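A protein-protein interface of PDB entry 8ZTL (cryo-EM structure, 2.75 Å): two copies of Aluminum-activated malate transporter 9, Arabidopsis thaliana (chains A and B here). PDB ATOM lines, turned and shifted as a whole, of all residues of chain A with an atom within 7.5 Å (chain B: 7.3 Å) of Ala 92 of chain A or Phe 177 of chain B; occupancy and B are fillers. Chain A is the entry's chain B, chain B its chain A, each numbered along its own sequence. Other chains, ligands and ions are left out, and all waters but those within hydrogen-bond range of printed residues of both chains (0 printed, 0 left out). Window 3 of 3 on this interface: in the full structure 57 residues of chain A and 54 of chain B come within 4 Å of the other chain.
The backbone carbonyl oxygen of Gly 180 of chain B is in hydrogen-bond range of the side-chain hydroxyl of Thr 184 of chain B, at 2.7 Å.
The backbone carbonyl oxygen (O) of Lys 87 of chain A is in hydrogen-bond range of the side-chain hydroxyl (OG) of Ser 91 of chain A, at 2.8 Å.
O of Gly 95 of chain A is in hydrogen-bond range of OG1 of Thr 99 of chain A, 3.1 Å away.
Phe 181 of chain B touches Ile 88 of chain A.
Phe 90 of chain A touches Thr 184 of chain B.
Phe 181 of chain B touches Ser 91 of chain A.
Ser 91 of chain A touches Thr 184 of chain B (OG to CB, 3.9 Å).
CE1 of Phe 177 of chain B touches O of Ala 92 of chain A (3.99 Å).
Ala 92 of chain A touches Phe 181 of chain B (N to CD2, 3.7 Å).
Phe 177 of chain B touches Gly 95 of chain A (CD1 to C, 3.5 Å).
Phe 177 of chain B touches Leu 96 of chain A.
Thr 99 of chain A touches Phe 177 of chain B.
Ala 102 of chain A touches Ile 176 of chain B (CB to CD1, 3.8 Å).
Of the printed residues of chain B, Ala 92 of chain A touches Phe 177 (3.99 Å) and Phe 181 (3.7 Å).
Printed residues of chain A within 4 Å of Phe 177 of chain B: Ala 92 (3.99 Å), Gly 95 (3.5 Å), Leu 96 (3.99 Å) and Thr 99 (3.2 Å).
Of the printed residues of chain A, Phe 181 of chain B touches Ile 88 (3.8 Å), Ser 91 (3.5 Å) and Ala 92 (3.7 Å).
Of the printed residues of chain B, Gly 95 of chain A touches Phe 177 (3.5 Å).
Printed residues of chain B within 4 Å of Leu 96 of chain A: Phe 177 (3.99 Å).
Gly 180 of chain B touches none of the printed residues of chain A.
The nearest printed residue of chain A that does not touch Phe 177 of chain B is Ser 91 of chain A (5.5 Å).
Hydrophobic or aromatic side chains of chain A that line the printed part of chain B: Phe 90 and Ala 102.
Of the 16 printed residues of chain B, 5 touch a printed residue of chain A.
Printed residues of chain B that touch a printed residue of chain A: Thr 173, Ile 176, Phe 177, Phe 181 and Thr 184.
Hydrophobic or aromatic side chains of chain B within 4 Å of the printed part of chain A: Ile 176, Phe 177 and Phe 181.
Among the printed residues, no Asp or Glu carboxylate lies within 4 Å of a Lys or Arg side-chain nitrogen of the other chain.
No position is printed for both chains.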
ATOM      1  N   ARG A  86     -11.540 -20.806   3.634  1.00  0.00           N
ATOM      2  CA  ARG A  86     -12.984 -20.725   3.426  1.00  0.00           C
ATOM      3  C   ARG A  86     -13.348 -20.931   1.957  1.00  0.00           C
ATOM      4  O   ARG A  86     -14.345 -21.599   1.636  1.00  0.00           O
ATOM      5  CB  ARG A  86     -13.481 -19.372   3.934  1.00  0.00           C
ATOM      6  CG  ARG A  86     -14.801 -19.402   4.677  1.00  0.00           C
ATOM      7  CD  ARG A  86     -14.969 -18.141   5.513  1.00  0.00           C
ATOM      8  NE  ARG A  86     -14.848 -16.923   4.720  1.00  0.00           N
ATOM      9  CZ  ARG A  86     -15.300 -15.735   5.097  1.00  0.00           C
ATOM     10  NH1 ARG A  86     -15.913 -15.565   6.256  1.00  0.00           N
ATOM     11  NH2 ARG A  86     -15.129 -14.691   4.291  1.00  0.00           N
ATOM     12  N   LYS A  87     -12.537 -20.380   1.052  1.00  0.00           N
ATOM     13  CA  LYS A  87     -12.806 -20.495  -0.376  1.00  0.00           C
ATOM     14  C   LYS A  87     -12.708 -21.940  -0.854  1.00  0.00           C
ATOM     15  O   LYS A  87     -13.469 -22.362  -1.733  1.00  0.00           O
ATOM     16  CB  LYS A  87     -11.836 -19.603  -1.149  1.00  0.00           C
ATOM     17  CG  LYS A  87     -11.911 -18.145  -0.740  1.00  0.00           C
ATOM     18  CD  LYS A  87     -10.774 -17.333  -1.328  1.00  0.00           C
ATOM     19  CE  LYS A  87     -11.234 -15.932  -1.683  1.00  0.00           C
ATOM     20  NZ  LYS A  87     -10.094 -15.040  -2.026  1.00  0.00           N
ATOM     21  N   ILE A  88     -11.786 -22.715  -0.285  1.00  0.00           N
ATOM     22  CA  ILE A  88     -11.667 -24.115  -0.674  1.00  0.00           C
ATOM     23  C   ILE A  88     -12.921 -24.885  -0.286  1.00  0.00           C
ATOM     24  O   ILE A  88     -13.416 -25.728  -1.049  1.00  0.00           O
ATOM     25  CB  ILE A  88     -10.406 -24.730  -0.043  1.00  0.00           C
ATOM     26  CG1 ILE A  88      -9.153 -24.259  -0.785  1.00  0.00           C
ATOM     27  CG2 ILE A  88     -10.503 -26.244  -0.031  1.00  0.00           C
ATOM     28  CD1 ILE A  88      -7.916 -24.205   0.078  1.00  0.00           C
ATOM     29  N   VAL A  89     -13.494 -24.566   0.877  1.00  0.00           N
ATOM     30  CA  VAL A  89     -14.719 -25.227   1.308  1.00  0.00           C
ATOM     31  C   VAL A  89     -15.878 -24.835   0.404  1.00  0.00           C
ATOM     32  O   VAL A  89     -16.694 -25.680   0.018  1.00  0.00           O
ATOM     33  CB  VAL A  89     -15.014 -24.901   2.783  1.00  0.00           C
ATOM     34  CG1 VAL A  89     -16.359 -25.475   3.196  1.00  0.00           C
ATOM     35  CG2 VAL A  89     -13.907 -25.433   3.680  1.00  0.00           C
ATOM     36  N   PHE A  90     -15.958 -23.555   0.034  1.00  0.00           N
ATOM     37  CA  PHE A  90     -17.033 -23.118  -0.852  1.00  0.00           C
ATOM     38  C   PHE A  90     -16.949 -23.814  -2.209  1.00  0.00           C
ATOM     39  O   PHE A  90     -17.967 -24.270  -2.757  1.00  0.00           O
ATOM     40  CB  PHE A  90     -16.975 -21.598  -1.009  1.00  0.00           C
ATOM     41  CG  PHE A  90     -18.079 -21.028  -1.843  1.00  0.00           C
ATOM     42  CD1 PHE A  90     -19.359 -20.915  -1.336  1.00  0.00           C
ATOM     43  CD2 PHE A  90     -17.833 -20.590  -3.132  1.00  0.00           C
ATOM     44  CE1 PHE A  90     -20.374 -20.388  -2.104  1.00  0.00           C
ATOM     45  CE2 PHE A  90     -18.846 -20.061  -3.901  1.00  0.00           C
ATOM     46  CZ  PHE A  90     -20.117 -19.959  -3.388  1.00  0.00           C
ATOM     47  N   SER A  91     -15.737 -23.928  -2.757  1.00  0.00           N
ATOM     48  CA  SER A  91     -15.574 -24.564  -4.061  1.00  0.00           C
ATOM     49  C   SER A  91     -15.900 -26.052  -3.999  1.00  0.00           C
ATOM     50  O   SER A  91     -16.534 -26.596  -4.917  1.00  0.00           O
ATOM     51  CB  SER A  91     -14.152 -24.343  -4.569  1.00  0.00           C
ATOM     52  OG  SER A  91     -13.791 -22.979  -4.472  1.00  0.00           O
ATOM     53  N   ALA A  92     -15.531 -26.722  -2.904  1.00  0.00           N
ATOM     54  CA  ALA A  92     -15.856 -28.138  -2.803  1.00  0.00           C
ATOM     55  C   ALA A  92     -17.344 -28.348  -2.567  1.00  0.00           C
ATOM     56  O   ALA A  92     -17.905 -29.356  -3.011  1.00  0.00           O
ATOM     57  CB  ALA A  92     -15.044 -28.789  -1.686  1.00  0.00           C
ATOM     58  N   LYS A  93     -18.020 -27.370  -1.963  1.00  0.00           N
ATOM     59  CA  LYS A  93     -19.461 -27.494  -1.773  1.00  0.00           C
ATOM     60  C   LYS A  93     -20.200 -27.354  -3.098  1.00  0.00           C
ATOM     61  O   LYS A  93     -21.139 -28.113  -3.379  1.00  0.00           O
ATOM     62  CB  LYS A  93     -19.945 -26.443  -0.775  1.00  0.00           C
ATOM     63  CG  LYS A  93     -19.540 -26.720   0.657  1.00  0.00           C
ATOM     64  CD  LYS A  93     -20.544 -26.154   1.635  1.00  0.00           C
ATOM     65  CE  LYS A  93     -20.654 -24.652   1.502  1.00  0.00           C
ATOM     66  NZ  LYS A  93     -21.140 -24.037   2.757  1.00  0.00           N
ATOM     67  N   ILE A  94     -19.781 -26.402  -3.932  1.00  0.00           N
ATOM     68  CA  ILE A  94     -20.416 -26.272  -5.242  1.00  0.00           C
ATOM     69  C   ILE A  94     -20.147 -27.509  -6.094  1.00  0.00           C
ATOM     70  O   ILE A  94     -21.049 -28.024  -6.778  1.00  0.00           O
ATOM     71  CB  ILE A  94     -19.948 -24.985  -5.943  1.00  0.00           C
ATOM     72  CG1 ILE A  94     -20.331 -23.762  -5.118  1.00  0.00           C
ATOM     73  CG2 ILE A  94     -20.557 -24.883  -7.327  1.00  0.00           C
ATOM     74  CD1 ILE A  94     -20.528 -22.526  -5.945  1.00  0.00           C
ATOM     75  N   GLY A  95     -18.911 -28.024  -6.056  1.00  0.00           N
ATOM     76  CA  GLY A  95     -18.621 -29.233  -6.805  1.00  0.00           C
ATOM     77  C   GLY A  95     -19.395 -30.436  -6.307  1.00  0.00           C
ATOM     78  O   GLY A  95     -19.771 -31.306  -7.097  1.00  0.00           O
ATOM     79  N   LEU A  96     -19.737 -30.456  -5.018  1.00  0.00           N
ATOM     80  CA  LEU A  96     -20.500 -31.583  -4.494  1.00  0.00           C
ATOM     81  C   LEU A  96     -21.969 -31.489  -4.881  1.00  0.00           C
ATOM     82  O   LEU A  96     -22.600 -32.511  -5.179  1.00  0.00           O
ATOM     83  CB  LEU A  96     -20.359 -31.655  -2.976  1.00  0.00           C
ATOM     84  CG  LEU A  96     -21.111 -32.803  -2.305  1.00  0.00           C
ATOM     85  CD1 LEU A  96     -20.402 -34.115  -2.568  1.00  0.00           C
ATOM     86  CD2 LEU A  96     -21.255 -32.555  -0.815  1.00  0.00           C
ATOM     87  N   ALA A  97     -22.530 -30.279  -4.899  1.00  0.00           N
ATOM     88  CA  ALA A  97     -23.906 -30.139  -5.369  1.00  0.00           C
ATOM     89  C   ALA A  97     -24.023 -30.546  -6.834  1.00  0.00           C
ATOM     90  O   ALA A  97     -24.963 -31.266  -7.224  1.00  0.00           O
ATOM     91  CB  ALA A  97     -24.389 -28.704  -5.164  1.00  0.00           C
ATOM     92  N   LEU A  98     -23.050 -30.138  -7.655  1.00  0.00           N
ATOM     93  CA  LEU A  98     -23.090 -30.542  -9.056  1.00  0.00           C
ATOM     94  C   LEU A  98     -22.914 -32.050  -9.200  1.00  0.00           C
ATOM     95  O   LEU A  98     -23.576 -32.679 -10.034  1.00  0.00           O
ATOM     96  CB  LEU A  98     -22.024 -29.796  -9.857  1.00  0.00           C
ATOM     97  CG  LEU A  98     -22.403 -28.411 -10.383  1.00  0.00           C
ATOM     98  CD1 LEU A  98     -21.163 -27.609 -10.721  1.00  0.00           C
ATOM     99  CD2 LEU A  98     -23.305 -28.530 -11.594  1.00  0.00           C
ATOM    100  N   THR A  99     -22.061 -32.656  -8.369  1.00  0.00           N
ATOM    101  CA  THR A  99     -21.872 -34.101  -8.441  1.00  0.00           C
ATOM    102  C   THR A  99     -23.146 -34.847  -8.064  1.00  0.00           C
ATOM    103  O   THR A  99     -23.476 -35.867  -8.679  1.00  0.00           O
ATOM    104  CB  THR A  99     -20.720 -34.526  -7.538  1.00  0.00           C
ATOM    105  OG1 THR A  99     -19.476 -34.242  -8.188  1.00  0.00           O
ATOM    106  CG2 THR A  99     -20.800 -36.011  -7.242  1.00  0.00           C
ATOM    107  N   ALA A 102     -25.612 -34.593 -10.921  1.00  0.00           N
ATOM    108  CA  ALA A 102     -25.127 -35.419 -12.021  1.00  0.00           C
ATOM    109  C   ALA A 102     -25.410 -36.893 -11.767  1.00  0.00           C
ATOM    110  O   ALA A 102     -25.865 -37.609 -12.663  1.00  0.00           O
ATOM    111  CB  ALA A 102     -23.632 -35.188 -12.236  1.00  0.00           C
ATOM    112  N   PHE A 129     -26.323 -20.735  -6.415  1.00  0.00           N
ATOM    113  CA  PHE A 129     -25.370 -21.010  -5.334  1.00  0.00           C
ATOM    114  C   PHE A 129     -24.543 -19.762  -5.032  1.00  0.00           C
ATOM    115  O   PHE A 129     -23.613 -19.427  -5.768  1.00  0.00           O
ATOM    116  CB  PHE A 129     -24.474 -22.182  -5.720  1.00  0.00           C
ATOM    117  CG  PHE A 129     -24.151 -23.113  -4.585  1.00  0.00           C
ATOM    118  CD1 PHE A 129     -23.281 -22.733  -3.582  1.00  0.00           C
ATOM    119  CD2 PHE A 129     -24.699 -24.379  -4.538  1.00  0.00           C
ATOM    120  CE1 PHE A 129     -22.977 -23.593  -2.550  1.00  0.00           C
ATOM    121  CE2 PHE A 129     -24.399 -25.239  -3.506  1.00  0.00           C
ATOM    122  CZ  PHE A 129     -23.540 -24.847  -2.512  1.00  0.00           C
ATOM    123  N   VAL A 240     -27.493 -28.072   0.462  1.00  0.00           N
ATOM    124  CA  VAL A 240     -26.046 -28.227   0.550  1.00  0.00           C
ATOM    125  C   VAL A 240     -25.409 -26.983   1.151  1.00  0.00           C
ATOM    126  O   VAL A 240     -24.506 -27.081   1.989  1.00  0.00           O
ATOM    127  CB  VAL A 240     -25.451 -28.559  -0.831  1.00  0.00           C
ATOM    128  CG1 VAL A 240     -23.939 -28.605  -0.750  1.00  0.00           C
ATOM    129  CG2 VAL A 240     -25.981 -29.882  -1.326  1.00  0.00           C
ATOM    130  N   PHE B 171     -16.626 -41.769 -14.120  1.00  0.00           N
ATOM    131  CA  PHE B 171     -15.623 -40.879 -14.693  1.00  0.00           C
ATOM    132  C   PHE B 171     -16.244 -39.532 -15.053  1.00  0.00           C
ATOM    133  O   PHE B 171     -15.643 -38.477 -14.814  1.00  0.00           O
ATOM    134  CB  PHE B 171     -14.981 -41.548 -15.913  1.00  0.00           C
ATOM    135  CG  PHE B 171     -13.755 -40.839 -16.452  1.00  0.00           C
ATOM    136  CD1 PHE B 171     -13.548 -39.482 -16.258  1.00  0.00           C
ATOM    137  CD2 PHE B 171     -12.802 -41.550 -17.157  1.00  0.00           C
ATOM    138  CE1 PHE B 171     -12.425 -38.856 -16.756  1.00  0.00           C
ATOM    139  CE2 PHE B 171     -11.678 -40.927 -17.656  1.00  0.00           C
ATOM    140  CZ  PHE B 171     -11.490 -39.578 -17.455  1.00  0.00           C
ATOM    141  N   CYS B 172     -17.454 -39.540 -15.619  1.00  0.00           N
ATOM    142  CA  CYS B 172     -18.097 -38.279 -15.972  1.00  0.00           C
ATOM    143  C   CYS B 172     -18.341 -37.409 -14.741  1.00  0.00           C
ATOM    144  O   CYS B 172     -18.081 -36.196 -14.762  1.00  0.00           O
ATOM    145  CB  CYS B 172     -19.407 -38.549 -16.710  1.00  0.00           C
ATOM    146  SG  CYS B 172     -19.198 -39.242 -18.366  1.00  0.00           S
ATOM    147  N   THR B 173     -18.824 -38.007 -13.648  1.00  0.00           N
ATOM    148  CA  THR B 173     -19.076 -37.215 -12.448  1.00  0.00           C
ATOM    149  C   THR B 173     -17.779 -36.769 -11.781  1.00  0.00           C
ATOM    150  O   THR B 173     -17.718 -35.664 -11.224  1.00  0.00           O
ATOM    151  CB  THR B 173     -19.944 -38.001 -11.467  1.00  0.00           C
ATOM    152  OG1 THR B 173     -19.949 -37.335 -10.199  1.00  0.00           O
ATOM    153  CG2 THR B 173     -19.414 -39.407 -11.289  1.00  0.00           C
ATOM    154  N   LEU B 174     -16.727 -37.591 -11.848  1.00  0.00           N
ATOM    155  CA  LEU B 174     -15.429 -37.153 -11.353  1.00  0.00           C
ATOM    156  C   LEU B 174     -14.848 -36.031 -12.197  1.00  0.00           C
ATOM    157  O   LEU B 174     -14.012 -35.269 -11.702  1.00  0.00           O
ATOM    158  CB  LEU B 174     -14.453 -38.328 -11.311  1.00  0.00           C
ATOM    159  CG  LEU B 174     -14.401 -39.167 -10.036  1.00  0.00           C
ATOM    160  CD1 LEU B 174     -13.836 -38.340  -8.894  1.00  0.00           C
ATOM    161  CD2 LEU B 174     -15.771 -39.702  -9.680  1.00  0.00           C
ATOM    162  N   SER B 175     -15.269 -35.915 -13.456  1.00  0.00           N
ATOM    163  CA  SER B 175     -14.854 -34.779 -14.270  1.00  0.00           C
ATOM    164  C   SER B 175     -15.638 -33.525 -13.908  1.00  0.00           C
ATOM    165  O   SER B 175     -15.071 -32.424 -13.834  1.00  0.00           O
ATOM    166  CB  SER B 175     -15.041 -35.108 -15.749  1.00  0.00           C
ATOM    167  OG  SER B 175     -14.019 -35.968 -16.213  1.00  0.00           O
ATOM    168  N   ILE B 176     -16.935 -33.687 -13.628  1.00  0.00           N
ATOM    169  CA  ILE B 176     -17.769 -32.531 -13.306  1.00  0.00           C
ATOM    170  C   ILE B 176     -17.356 -31.929 -11.970  1.00  0.00           C
ATOM    171  O   ILE B 176     -17.303 -30.700 -11.819  1.00  0.00           O
ATOM    172  CB  ILE B 176     -19.258 -32.919 -13.308  1.00  0.00           C
ATOM    173  CG1 ILE B 176     -19.711 -33.318 -14.713  1.00  0.00           C
ATOM    174  CG2 ILE B 176     -20.102 -31.777 -12.773  1.00  0.00           C
ATOM    175  CD1 ILE B 176     -20.863 -34.287 -14.726  1.00  0.00           C
ATOM    176  N   PHE B 177     -17.032 -32.775 -10.989  1.00  0.00           N
ATOM    177  CA  PHE B 177     -16.626 -32.256  -9.684  1.00  0.00           C
ATOM    178  C   PHE B 177     -15.348 -31.431  -9.795  1.00  0.00           C
ATOM    179  O   PHE B 177     -15.262 -30.312  -9.265  1.00  0.00           O
ATOM    180  CB  PHE B 177     -16.440 -33.415  -8.703  1.00  0.00           C
ATOM    181  CG  PHE B 177     -15.805 -33.015  -7.400  1.00  0.00           C
ATOM    182  CD1 PHE B 177     -16.556 -32.441  -6.391  1.00  0.00           C
ATOM    183  CD2 PHE B 177     -14.453 -33.220  -7.183  1.00  0.00           C
ATOM    184  CE1 PHE B 177     -15.970 -32.075  -5.196  1.00  0.00           C
ATOM    185  CE2 PHE B 177     -13.864 -32.856  -5.989  1.00  0.00           C
ATOM    186  CZ  PHE B 177     -14.622 -32.281  -4.997  1.00  0.00           C
ATOM    187  N   CYS B 178     -14.358 -31.949 -10.521  1.00  0.00           N
ATOM    188  CA  CYS B 178     -13.088 -31.245 -10.649  1.00  0.00           C
ATOM    189  C   CYS B 178     -13.256 -29.943 -11.417  1.00  0.00           C
ATOM    190  O   CYS B 178     -12.661 -28.919 -11.051  1.00  0.00           O
ATOM    191  CB  CYS B 178     -12.059 -32.141 -11.332  1.00  0.00           C
ATOM    192  SG  CYS B 178     -11.517 -33.550 -10.346  1.00  0.00           S
ATOM    193  N   ILE B 179     -14.078 -29.950 -12.468  1.00  0.00           N
ATOM    194  CA  ILE B 179     -14.243 -28.736 -13.257  1.00  0.00           C
ATOM    195  C   ILE B 179     -14.958 -27.663 -12.447  1.00  0.00           C
ATOM    196  O   ILE B 179     -14.577 -26.485 -12.483  1.00  0.00           O
ATOM    197  CB  ILE B 179     -14.978 -29.042 -14.571  1.00  0.00           C
ATOM    198  CG1 ILE B 179     -14.212 -30.095 -15.365  1.00  0.00           C
ATOM    199  CG2 ILE B 179     -15.135 -27.782 -15.394  1.00  0.00           C
ATOM    200  CD1 ILE B 179     -12.804 -29.683 -15.709  1.00  0.00           C
ATOM    201  N   GLY B 180     -15.984 -28.045 -11.682  1.00  0.00           N
ATOM    202  CA  GLY B 180     -16.660 -27.058 -10.859  1.00  0.00           C
ATOM    203  C   GLY B 180     -15.758 -26.486  -9.783  1.00  0.00           C
ATOM    204  O   GLY B 180     -15.752 -25.272  -9.543  1.00  0.00           O
ATOM    205  N   PHE B 181     -14.923 -27.335  -9.175  1.00  0.00           N
ATOM    206  CA  PHE B 181     -14.039 -26.838  -8.127  1.00  0.00           C
ATOM    207  C   PHE B 181     -12.997 -25.881  -8.695  1.00  0.00           C
ATOM    208  O   PHE B 181     -12.739 -24.816  -8.116  1.00  0.00           O
ATOM    209  CB  PHE B 181     -13.358 -28.007  -7.412  1.00  0.00           C
ATOM    210  CG  PHE B 181     -12.322 -27.583  -6.409  1.00  0.00           C
ATOM    211  CD1 PHE B 181     -11.024 -27.305  -6.806  1.00  0.00           C
ATOM    212  CD2 PHE B 181     -12.646 -27.458  -5.073  1.00  0.00           C
ATOM    213  CE1 PHE B 181     -10.075 -26.906  -5.891  1.00  0.00           C
ATOM    214  CE2 PHE B 181     -11.700 -27.061  -4.151  1.00  0.00           C
ATOM    215  CZ  PHE B 181     -10.413 -26.785  -4.561  1.00  0.00           C
ATOM    216  N   LEU B 182     -12.433 -26.209  -9.860  1.00  0.00           N
ATOM    217  CA  LEU B 182     -11.398 -25.348 -10.418  1.00  0.00           C
ATOM    218  C   LEU B 182     -11.982 -24.037 -10.916  1.00  0.00           C
ATOM    219  O   LEU B 182     -11.377 -22.975 -10.726  1.00  0.00           O
ATOM    220  CB  LEU B 182     -10.658 -26.067 -11.545  1.00  0.00           C
ATOM    221  CG  LEU B 182      -9.503 -26.969 -11.110  1.00  0.00           C
ATOM    222  CD1 LEU B 182      -9.074 -27.886 -12.238  1.00  0.00           C
ATOM    223  CD2 LEU B 182      -8.337 -26.130 -10.623  1.00  0.00           C
ATOM    224  N   ALA B 183     -13.180 -24.071 -11.506  1.00  0.00           N
ATOM    225  CA  ALA B 183     -13.764 -22.830 -11.997  1.00  0.00           C
ATOM    226  C   ALA B 183     -14.153 -21.907 -10.850  1.00  0.00           C
ATOM    227  O   ALA B 183     -13.930 -20.692 -10.925  1.00  0.00           O
ATOM    228  CB  ALA B 183     -14.971 -23.129 -12.884  1.00  0.00           C
ATOM    229  N   THR B 184     -14.662 -22.461  -9.743  1.00  0.00           N
ATOM    230  CA  THR B 184     -15.036 -21.582  -8.638  1.00  0.00           C
ATOM    231  C   THR B 184     -13.803 -21.006  -7.953  1.00  0.00           C
ATOM    232  O   THR B 184     -13.747 -19.799  -7.666  1.00  0.00           O
ATOM    233  CB  THR B 184     -15.904 -22.332  -7.631  1.00  0.00           C
ATOM    234  OG1 THR B 184     -16.871 -23.122  -8.331  1.00  0.00           O
ATOM    235  CG2 THR B 184     -16.630 -21.351  -6.730  1.00  0.00           C
ATOM    236  N   LEU B 203     -18.177 -23.020 -17.269  1.00  0.00           N
ATOM    237  CA  LEU B 203     -18.762 -24.117 -16.511  1.00  0.00           C
ATOM    238  C   LEU B 203     -20.108 -24.528 -17.092  1.00  0.00           C
ATOM    239  O   LEU B 203     -20.401 -25.727 -17.211  1.00  0.00           O
ATOM    240  CB  LEU B 203     -18.890 -23.718 -15.040  1.00  0.00           C
ATOM    241  CG  LEU B 203     -19.292 -24.790 -14.023  1.00  0.00           C
ATOM    242  CD1 LEU B 203     -18.472 -26.050 -14.210  1.00  0.00           C
ATOM    243  CD2 LEU B 203     -19.143 -24.269 -12.611  1.00  0.00           C
ATOM    244  N   TYR B 206     -19.495 -26.554 -20.297  1.00  0.00           N
ATOM    245  CA  TYR B 206     -18.977 -27.889 -20.018  1.00  0.00           C
ATOM    246  C   TYR B 206     -20.086 -28.811 -19.533  1.00  0.00           C
ATOM    247  O   TYR B 206     -20.248 -29.931 -20.034  1.00  0.00           O
ATOM    248  CB  TYR B 206     -17.857 -27.811 -18.984  1.00  0.00           C
ATOM    249  CG  TYR B 206     -17.095 -29.104 -18.813  1.00  0.00           C
ATOM    250  CD1 TYR B 206     -16.040 -29.425 -19.650  1.00  0.00           C
ATOM    251  CD2 TYR B 206     -17.437 -30.008 -17.818  1.00  0.00           C
ATOM    252  CE1 TYR B 206     -15.346 -30.604 -19.499  1.00  0.00           C
ATOM    253  CE2 TYR B 206     -16.748 -31.188 -17.659  1.00  0.00           C
ATOM    254  CZ  TYR B 206     -15.702 -31.482 -18.503  1.00  0.00           C
ATOM    255  OH  TYR B 206     -15.009 -32.659 -18.354  1.00  0.00           O
